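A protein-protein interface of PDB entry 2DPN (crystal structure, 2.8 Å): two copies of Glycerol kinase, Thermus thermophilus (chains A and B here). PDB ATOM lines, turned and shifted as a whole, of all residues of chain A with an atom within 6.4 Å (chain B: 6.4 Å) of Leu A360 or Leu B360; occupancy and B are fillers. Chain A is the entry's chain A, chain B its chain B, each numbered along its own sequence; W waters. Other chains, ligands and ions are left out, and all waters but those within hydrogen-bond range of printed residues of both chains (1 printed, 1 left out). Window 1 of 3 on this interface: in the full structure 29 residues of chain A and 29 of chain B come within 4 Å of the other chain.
Among the printed residues, merely in contact across the chains: Leu A318 with Leu B318, Gly A358 with Leu B361, Thr A359 with Leu B360, Thr A359 with Leu B361, Leu A360 with Gly B358, Leu A360 with Thr B359, Leu A361 with Thr B359 and Leu A363 with Trp B312.
Of the 14 printed residues of chain B, 8 touch a printed residue of chain A.
Printed residues of chain B that touch a printed residue of chain A: Trp B312, Leu B318, Gly B358, Thr B359, Leu B360, Leu B361, Gly B362 and Leu B363.
Hydrophobic or aromatic side chains of chain B within 4 Å of the printed part of chain A: Trp B312, Leu B318, Leu B360, Leu B361 and Leu B363.
Hydrophobic or aromatic side chains of chain A within 4 Å of the printed part of chain B: Leu A318, Leu A360, Leu A361 and Leu A363.
Along chain A the printed residues that touch a printed residue of chain B span positions 318 to 363.
Among the printed residues, 13 pairs touch across the chains.
Among the printed residues, no Asp or Glu carboxylate lies within 4 Å of a Lys or Arg side-chain nitrogen of the other chain.
Of the printed residues of chain B, Leu A360 touches Gly B358 (3.8 Å), Thr B359 (3.3 Å) and Leu B360 (3.1 Å).
Of chain A, only Thr A359 (3.4 Å) and Leu A360 (3.1 Å) come within 4 Å of Leu B360.
Of the printed residues of chain B, Leu A361 touches Thr B359.
Printed residues of chain A within 4 Å of Leu B361: Gly A358 (3.9 Å) and Thr A359 (3.3 Å).
Of the printed residues of chain A, Trp B312 touches Leu A363 (3.8 Å).
Of the printed residues of chain A, Thr B359 touches Leu A360 and Leu A361.
Phe A340 touches none of the printed residues of chain B.
Val A338 touches none of the printed residues of chain B.
The nearest printed residue of chain B that does not touch Thr A359 is Leu B363 (4.4 Å).
Leu A318 touches its own counterpart, Leu B318.
Gly A358 touches Leu B363, and with the chains exchanged Leu A363 touches Gly B358.
Leu A360 touches Gly B358, but with the chains exchanged Gly A358 does not touch Leu B360 (4.1 Å).
Leu A360 touches its own counterpart, Leu B360.
Positions printed for both chains: 312, 318, 338, 339, 340, 341, 358, 359, 360, 361, 362, 363, 372 and 375.
Of the 13 pairs that touch across the chains among the printed residues, 10 have their exchanged pair printed and touching as well.
The backbone carbonyl oxygen (O) of Gly A358 lies within hydrogen-bond range of the backbone NH (N) of Gly B362.
N of Gly A358 lies within hydrogen-bond range of O of Leu B363 (3.0 Å).
O of Leu A360 is in hydrogen-bond range of N of Leu B360, at 3.1 Å.
O of Gly B358 lies within hydrogen-bond range of N of Gly A362.
N of Gly B358 is in hydrogen-bond range of O of Leu A363.
Water W1 lies within hydrogen-bond range of N of Gly A362 (2.6 Å), OG1 of Thr B359 (3.0 Å) and O of Gly B358 (3.4 Å).
The backbone NH (N) of Tyr A339 is in hydrogen-bond range of the backbone carbonyl oxygen (O) of Leu A361, 2.7 Å away.
N of Val A341 lies within hydrogen-bond range of O of Thr A359 (2.9 Å).
The backbone NH (N) of Leu B361 is in hydrogen-bond range of the backbone carbonyl oxygen (O) of Tyr B339, at 2.8 Å.
The backbone NH of Val B341 lies within hydrogen-bond range of the backbone carbonyl oxygen of Thr B359, at 2.7 Å.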
ATOM      1  N   TRP A 312      17.942 -24.527  27.071  1.00  0.00           N
ATOM      2  CA  TRP A 312      18.816 -24.560  28.231  1.00  0.00           C
ATOM      3  C   TRP A 312      19.929 -23.522  28.084  1.00  0.00           C
ATOM      4  O   TRP A 312      20.217 -22.764  29.011  1.00  0.00           O
ATOM      5  CB  TRP A 312      19.413 -25.960  28.407  1.00  0.00           C
ATOM      6  CG  TRP A 312      20.328 -26.022  29.574  1.00  0.00           C
ATOM      7  CD1 TRP A 312      19.977 -25.975  30.890  1.00  0.00           C
ATOM      8  CD2 TRP A 312      21.758 -26.011  29.538  1.00  0.00           C
ATOM      9  NE1 TRP A 312      21.098 -25.925  31.681  1.00  0.00           N
ATOM     10  CE2 TRP A 312      22.208 -25.949  30.875  1.00  0.00           C
ATOM     11  CE3 TRP A 312      22.703 -26.042  28.508  1.00  0.00           C
ATOM     12  CZ2 TRP A 312      23.571 -25.917  31.208  1.00  0.00           C
ATOM     13  CZ3 TRP A 312      24.052 -26.008  28.838  1.00  0.00           C
ATOM     14  CH2 TRP A 312      24.473 -25.947  30.177  1.00  0.00           C
ATOM     15  N   LEU A 318      23.825 -18.592  27.730  1.00  0.00           N
ATOM     16  CA  LEU A 318      24.895 -18.759  26.752  1.00  0.00           C
ATOM     17  C   LEU A 318      24.484 -18.126  25.423  1.00  0.00           C
ATOM     18  O   LEU A 318      25.316 -17.869  24.560  1.00  0.00           O
ATOM     19  CB  LEU A 318      25.243 -20.234  26.580  1.00  0.00           C
ATOM     20  CG  LEU A 318      26.385 -20.642  27.516  1.00  0.00           C
ATOM     21  CD1 LEU A 318      26.439 -22.149  27.669  1.00  0.00           C
ATOM     22  CD2 LEU A 318      27.695 -20.107  26.961  1.00  0.00           C
ATOM     23  N   VAL A 338      34.526 -30.419  20.365  1.00  0.00           N
ATOM     24  CA  VAL A 338      33.713 -30.311  21.555  1.00  0.00           C
ATOM     25  C   VAL A 338      32.352 -30.923  21.252  1.00  0.00           C
ATOM     26  O   VAL A 338      31.746 -30.633  20.219  1.00  0.00           O
ATOM     27  CB  VAL A 338      33.534 -28.855  21.945  1.00  0.00           C
ATOM     28  CG1 VAL A 338      32.621 -28.743  23.138  1.00  0.00           C
ATOM     29  CG2 VAL A 338      34.869 -28.254  22.254  1.00  0.00           C
ATOM     30  N   TYR A 339      31.880 -31.775  22.155  1.00  0.00           N
ATOM     31  CA  TYR A 339      30.606 -32.444  21.984  1.00  0.00           C
ATOM     32  C   TYR A 339      29.627 -32.145  23.086  1.00  0.00           C
ATOM     33  O   TYR A 339      29.997 -31.947  24.236  1.00  0.00           O
ATOM     34  CB  TYR A 339      30.838 -33.944  21.860  1.00  0.00           C
ATOM     35  CG  TYR A 339      31.410 -34.279  20.510  1.00  0.00           C
ATOM     36  CD1 TYR A 339      30.571 -34.609  19.443  1.00  0.00           C
ATOM     37  CD2 TYR A 339      32.773 -34.126  20.254  1.00  0.00           C
ATOM     38  CE1 TYR A 339      31.069 -34.765  18.153  1.00  0.00           C
ATOM     39  CE2 TYR A 339      33.285 -34.279  18.965  1.00  0.00           C
ATOM     40  CZ  TYR A 339      32.426 -34.593  17.920  1.00  0.00           C
ATOM     41  OH  TYR A 339      32.916 -34.698  16.640  1.00  0.00           O
ATOM     42  N   PHE A 340      28.359 -32.106  22.716  1.00  0.00           N
ATOM     43  CA  PHE A 340      27.300 -31.823  23.663  1.00  0.00           C
ATOM     44  C   PHE A 340      26.270 -32.939  23.535  1.00  0.00           C
ATOM     45  O   PHE A 340      25.678 -33.139  22.485  1.00  0.00           O
ATOM     46  CB  PHE A 340      26.688 -30.449  23.335  1.00  0.00           C
ATOM     47  CG  PHE A 340      25.653 -29.961  24.322  1.00  0.00           C
ATOM     48  CD1 PHE A 340      25.034 -28.731  24.123  1.00  0.00           C
ATOM     49  CD2 PHE A 340      25.260 -30.732  25.410  1.00  0.00           C
ATOM     50  CE1 PHE A 340      24.036 -28.274  24.984  1.00  0.00           C
ATOM     51  CE2 PHE A 340      24.259 -30.286  26.282  1.00  0.00           C
ATOM     52  CZ  PHE A 340      23.646 -29.054  26.067  1.00  0.00           C
ATOM     53  N   VAL A 341      26.090 -33.699  24.601  1.00  0.00           N
ATOM     54  CA  VAL A 341      25.108 -34.762  24.593  1.00  0.00           C
ATOM     55  C   VAL A 341      24.053 -34.222  25.539  1.00  0.00           C
ATOM     56  O   VAL A 341      24.191 -34.312  26.757  1.00  0.00           O
ATOM     57  CB  VAL A 341      25.685 -36.087  25.131  1.00  0.00           C
ATOM     58  CG1 VAL A 341      24.703 -37.215  24.877  1.00  0.00           C
ATOM     59  CG2 VAL A 341      27.005 -36.387  24.457  1.00  0.00           C
ATOM     60  N   GLY A 358      23.199 -34.708  30.966  1.00  0.00           N
ATOM     61  CA  GLY A 358      23.755 -33.737  30.036  1.00  0.00           C
ATOM     62  C   GLY A 358      25.256 -33.666  30.189  1.00  0.00           C
ATOM     63  O   GLY A 358      25.750 -33.415  31.283  1.00  0.00           O
ATOM     64  N   THR A 359      25.984 -33.857  29.095  1.00  0.00           N
ATOM     65  CA  THR A 359      27.442 -33.874  29.157  1.00  0.00           C
ATOM     66  C   THR A 359      28.144 -33.070  28.076  1.00  0.00           C
ATOM     67  O   THR A 359      27.856 -33.228  26.899  1.00  0.00           O
ATOM     68  CB  THR A 359      27.982 -35.327  29.025  1.00  0.00           C
ATOM     69  OG1 THR A 359      27.262 -36.209  29.900  1.00  0.00           O
ATOM     70  CG2 THR A 359      29.460 -35.374  29.363  1.00  0.00           C
ATOM     71  N   LEU A 360      29.091 -32.230  28.477  1.00  0.00           N
ATOM     72  CA  LEU A 360      29.875 -31.445  27.530  1.00  0.00           C
ATOM     73  C   LEU A 360      31.292 -32.016  27.541  1.00  0.00           C
ATOM     74  O   LEU A 360      31.916 -32.139  28.599  1.00  0.00           O
ATOM     75  CB  LEU A 360      29.898 -29.976  27.941  1.00  0.00           C
ATOM     76  CG  LEU A 360      29.372 -29.002  26.885  1.00  0.00           C
ATOM     77  CD1 LEU A 360      27.903 -29.271  26.609  1.00  0.00           C
ATOM     78  CD2 LEU A 360      29.560 -27.589  27.381  1.00  0.00           C
ATOM     79  N   LEU A 361      31.791 -32.371  26.362  1.00  0.00           N
ATOM     80  CA  LEU A 361      33.117 -32.956  26.238  1.00  0.00           C
ATOM     81  C   LEU A 361      34.024 -32.203  25.285  1.00  0.00           C
ATOM     82  O   LEU A 361      33.567 -31.666  24.282  1.00  0.00           O
ATOM     83  CB  LEU A 361      32.991 -34.389  25.750  1.00  0.00           C
ATOM     84  CG  LEU A 361      32.186 -35.294  26.672  1.00  0.00           C
ATOM     85  CD1 LEU A 361      31.721 -36.511  25.905  1.00  0.00           C
ATOM     86  CD2 LEU A 361      33.039 -35.690  27.858  1.00  0.00           C
ATOM     87  N   GLY A 362      35.316 -32.178  25.608  1.00  0.00           N
ATOM     88  CA  GLY A 362      36.296 -31.513  24.766  1.00  0.00           C
ATOM     89  C   GLY A 362      36.457 -30.024  24.974  1.00  0.00           C
ATOM     90  O   GLY A 362      36.908 -29.321  24.081  1.00  0.00           O
ATOM     91  N   LEU A 363      36.098 -29.518  26.141  1.00  0.00           N
ATOM     92  CA  LEU A 363      36.245 -28.094  26.357  1.00  0.00           C
ATOM     93  C   LEU A 363      37.720 -27.760  26.455  1.00  0.00           C
ATOM     94  O   LEU A 363      38.497 -28.549  26.979  1.00  0.00           O
ATOM     95  CB  LEU A 363      35.525 -27.674  27.629  1.00  0.00           C
ATOM     96  CG  LEU A 363      34.016 -27.909  27.639  1.00  0.00           C
ATOM     97  CD1 LEU A 363      33.410 -27.221  28.862  1.00  0.00           C
ATOM     98  CD2 LEU A 363      33.392 -27.349  26.364  1.00  0.00           C
ATOM     99  N   LEU A 372      29.781 -23.780  21.404  1.00  0.00           N
ATOM    100  CA  LEU A 372      28.801 -24.494  22.212  1.00  0.00           C
ATOM    101  C   LEU A 372      27.469 -24.450  21.491  1.00  0.00           C
ATOM    102  O   LEU A 372      26.715 -25.425  21.492  1.00  0.00           O
ATOM    103  CB  LEU A 372      28.685 -23.866  23.604  1.00  0.00           C
ATOM    104  CG  LEU A 372      29.966 -23.956  24.442  1.00  0.00           C
ATOM    105  CD1 LEU A 372      29.712 -23.394  25.822  1.00  0.00           C
ATOM    106  CD2 LEU A 372      30.429 -25.400  24.550  1.00  0.00           C
ATOM    107  N   ALA A 375      27.699 -27.102  18.837  1.00  0.00           N
ATOM    108  CA  ALA A 375      27.682 -28.410  19.486  1.00  0.00           C
ATOM    109  C   ALA A 375      26.267 -28.839  19.888  1.00  0.00           C
ATOM    110  O   ALA A 375      25.905 -30.012  19.769  1.00  0.00           O
ATOM    111  CB  ALA A 375      28.592 -28.391  20.704  1.00  0.00           C
ATOM    112  N   TRP B 312      37.374 -19.035  31.936  1.00  0.00           N
ATOM    113  CA  TRP B 312      36.647 -19.553  30.798  1.00  0.00           C
ATOM    114  C   TRP B 312      35.171 -19.179  30.916  1.00  0.00           C
ATOM    115  O   TRP B 312      34.559 -18.763  29.938  1.00  0.00           O
ATOM    116  CB  TRP B 312      36.789 -21.072  30.704  1.00  0.00           C
ATOM    117  CG  TRP B 312      36.033 -21.648  29.545  1.00  0.00           C
ATOM    118  CD1 TRP B 312      36.376 -21.586  28.218  1.00  0.00           C
ATOM    119  CD2 TRP B 312      34.764 -22.294  29.599  1.00  0.00           C
ATOM    120  NE1 TRP B 312      35.395 -22.149  27.446  1.00  0.00           N
ATOM    121  CE2 TRP B 312      34.391 -22.593  28.266  1.00  0.00           C
ATOM    122  CE3 TRP B 312      33.903 -22.650  30.642  1.00  0.00           C
ATOM    123  CZ2 TRP B 312      33.192 -23.234  27.951  1.00  0.00           C
ATOM    124  CZ3 TRP B 312      32.713 -23.284  30.333  1.00  0.00           C
ATOM    125  CH2 TRP B 312      32.367 -23.572  28.995  1.00  0.00           C
ATOM    126  N   LEU B 318      28.976 -16.690  30.922  1.00  0.00           N
ATOM    127  CA  LEU B 318      28.176 -17.297  31.984  1.00  0.00           C
ATOM    128  C   LEU B 318      28.181 -16.402  33.216  1.00  0.00           C
ATOM    129  O   LEU B 318      27.367 -16.569  34.121  1.00  0.00           O
ATOM    130  CB  LEU B 318      28.688 -18.700  32.323  1.00  0.00           C
ATOM    131  CG  LEU B 318      28.565 -19.753  31.209  1.00  0.00           C
ATOM    132  CD1 LEU B 318      29.199 -21.056  31.660  1.00  0.00           C
ATOM    133  CD2 LEU B 318      27.108 -19.991  30.859  1.00  0.00           C
ATOM    134  N   VAL B 338      26.185 -31.566  39.575  1.00  0.00           N
ATOM    135  CA  VAL B 338      26.946 -31.165  38.404  1.00  0.00           C
ATOM    136  C   VAL B 338      28.429 -31.117  38.770  1.00  0.00           C
ATOM    137  O   VAL B 338      28.798 -30.746  39.888  1.00  0.00           O
ATOM    138  CB  VAL B 338      26.495 -29.787  37.882  1.00  0.00           C
ATOM    139  CG1 VAL B 338      27.370 -29.363  36.727  1.00  0.00           C
ATOM    140  CG2 VAL B 338      25.070 -29.864  37.411  1.00  0.00           C
ATOM    141  N   TYR B 339      29.274 -31.532  37.833  1.00  0.00           N
ATOM    142  CA  TYR B 339      30.704 -31.550  38.062  1.00  0.00           C
ATOM    143  C   TYR B 339      31.398 -31.010  36.844  1.00  0.00           C
ATOM    144  O   TYR B 339      31.102 -31.396  35.717  1.00  0.00           O
ATOM    145  CB  TYR B 339      31.159 -32.974  38.378  1.00  0.00           C
ATOM    146  CG  TYR B 339      30.656 -33.407  39.726  1.00  0.00           C
ATOM    147  CD1 TYR B 339      31.428 -33.222  40.867  1.00  0.00           C
ATOM    148  CD2 TYR B 339      29.350 -33.863  39.881  1.00  0.00           C
ATOM    149  CE1 TYR B 339      30.907 -33.469  42.132  1.00  0.00           C
ATOM    150  CE2 TYR B 339      28.819 -34.111  41.137  1.00  0.00           C
ATOM    151  CZ  TYR B 339      29.602 -33.911  42.260  1.00  0.00           C
ATOM    152  OH  TYR B 339      29.079 -34.171  43.509  1.00  0.00           O
ATOM    153  N   PHE B 340      32.314 -30.089  37.080  1.00  0.00           N
ATOM    154  CA  PHE B 340      33.041 -29.466  36.001  1.00  0.00           C
ATOM    155  C   PHE B 340      34.522 -29.777  36.162  1.00  0.00           C
ATOM    156  O   PHE B 340      35.155 -29.319  37.104  1.00  0.00           O
ATOM    157  CB  PHE B 340      32.785 -27.949  36.037  1.00  0.00           C
ATOM    158  CG  PHE B 340      33.490 -27.172  34.959  1.00  0.00           C
ATOM    159  CD1 PHE B 340      33.616 -25.794  35.066  1.00  0.00           C
ATOM    160  CD2 PHE B 340      34.052 -27.806  33.864  1.00  0.00           C
ATOM    161  CE1 PHE B 340      34.299 -25.061  34.101  1.00  0.00           C
ATOM    162  CE2 PHE B 340      34.734 -27.085  32.900  1.00  0.00           C
ATOM    163  CZ  PHE B 340      34.861 -25.712  33.015  1.00  0.00           C
ATOM    164  N   VAL B 341      35.054 -30.578  35.245  1.00  0.00           N
ATOM    165  CA  VAL B 341      36.467 -30.939  35.256  1.00  0.00           C
ATOM    166  C   VAL B 341      37.145 -30.009  34.248  1.00  0.00           C
ATOM    167  O   VAL B 341      37.107 -30.251  33.042  1.00  0.00           O
ATOM    168  CB  VAL B 341      36.654 -32.416  34.862  1.00  0.00           C
ATOM    169  CG1 VAL B 341      38.075 -32.861  35.146  1.00  0.00           C
ATOM    170  CG2 VAL B 341      35.663 -33.275  35.643  1.00  0.00           C
ATOM    171  N   GLY B 358      38.318 -30.333  29.194  1.00  0.00           N
ATOM    172  CA  GLY B 358      37.264 -29.755  30.005  1.00  0.00           C
ATOM    173  C   GLY B 358      35.980 -30.541  29.848  1.00  0.00           C
ATOM    174  O   GLY B 358      35.501 -30.749  28.730  1.00  0.00           O
ATOM    175  N   THR B 359      35.414 -30.961  30.977  1.00  0.00           N
ATOM    176  CA  THR B 359      34.202 -31.765  30.987  1.00  0.00           C
ATOM    177  C   THR B 359      33.146 -31.305  32.007  1.00  0.00           C
ATOM    178  O   THR B 359      33.465 -30.986  33.152  1.00  0.00           O
ATOM    179  CB  THR B 359      34.570 -33.235  31.295  1.00  0.00           C
ATOM    180  OG1 THR B 359      35.546 -33.684  30.355  1.00  0.00           O
ATOM    181  CG2 THR B 359      33.351 -34.130  31.245  1.00  0.00           C
ATOM    182  N   LEU B 360      31.888 -31.272  31.575  1.00  0.00           N
ATOM    183  CA  LEU B 360      30.779 -30.915  32.450  1.00  0.00           C
ATOM    184  C   LEU B 360      29.958 -32.178  32.590  1.00  0.00           C
ATOM    185  O   LEU B 360      29.833 -32.937  31.636  1.00  0.00           O
ATOM    186  CB  LEU B 360      29.917 -29.808  31.848  1.00  0.00           C
ATOM    187  CG  LEU B 360      30.306 -28.372  32.203  1.00  0.00           C
ATOM    188  CD1 LEU B 360      29.222 -27.420  31.695  1.00  0.00           C
ATOM    189  CD2 LEU B 360      30.445 -28.237  33.706  1.00  0.00           C
ATOM    190  N   LEU B 361      29.396 -32.413  33.770  1.00  0.00           N
ATOM    191  CA  LEU B 361      28.621 -33.623  33.979  1.00  0.00           C
ATOM    192  C   LEU B 361      27.366 -33.442  34.817  1.00  0.00           C
ATOM    193  O   LEU B 361      27.322 -32.603  35.714  1.00  0.00           O
ATOM    194  CB  LEU B 361      29.506 -34.688  34.627  1.00  0.00           C
ATOM    195  CG  LEU B 361      30.681 -35.156  33.775  1.00  0.00           C
ATOM    196  CD1 LEU B 361      31.598 -36.030  34.612  1.00  0.00           C
ATOM    197  CD2 LEU B 361      30.161 -35.919  32.551  1.00  0.00           C
ATOM    198  N   GLY B 362      26.349 -34.239  34.500  1.00  0.00           N
ATOM    199  CA  GLY B 362      25.105 -34.215  35.240  1.00  0.00           C
ATOM    200  C   GLY B 362      24.194 -33.035  35.020  1.00  0.00           C
ATOM    201  O   GLY B 362      23.436 -32.670  35.919  1.00  0.00           O
ATOM    202  N   LEU B 363      24.256 -32.435  33.837  1.00  0.00           N
ATOM    203  CA  LEU B 363      23.395 -31.298  33.533  1.00  0.00           C
ATOM    204  C   LEU B 363      21.963 -31.789  33.380  1.00  0.00           C
ATOM    205  O   LEU B 363      21.717 -32.859  32.835  1.00  0.00           O
ATOM    206  CB  LEU B 363      23.843 -30.619  32.242  1.00  0.00           C
ATOM    207  CG  LEU B 363      25.291 -30.127  32.183  1.00  0.00           C
ATOM    208  CD1 LEU B 363      25.609 -29.771  30.737  1.00  0.00           C
ATOM    209  CD2 LEU B 363      25.508 -28.928  33.121  1.00  0.00           C
ATOM    210  N   LEU B 372      26.613 -23.825  37.731  1.00  0.00           N
ATOM    211  CA  LEU B 372      27.831 -23.943  36.933  1.00  0.00           C
ATOM    212  C   LEU B 372      28.970 -23.176  37.590  1.00  0.00           C
ATOM    213  O   LEU B 372      30.133 -23.572  37.515  1.00  0.00           O
ATOM    214  CB  LEU B 372      27.592 -23.396  35.524  1.00  0.00           C
ATOM    215  CG  LEU B 372      26.545 -24.135  34.694  1.00  0.00           C
ATOM    216  CD1 LEU B 372      26.381 -23.457  33.342  1.00  0.00           C
ATOM    217  CD2 LEU B 372      26.981 -25.589  34.523  1.00  0.00           C
ATOM    218  N   ALA B 375      30.099 -25.221  40.483  1.00  0.00           N
ATOM    219  CA  ALA B 375      30.834 -26.364  39.960  1.00  0.00           C
ATOM    220  C   ALA B 375      32.273 -25.979  39.604  1.00  0.00           C
ATOM    221  O   ALA B 375      33.221 -26.697  39.930  1.00  0.00           O
ATOM    222  CB  ALA B 375      30.131 -26.927  38.737  1.00  0.00           C
HETATM  223  O   HOH W   1      36.015 -33.835  27.432  1.00  0.00           O
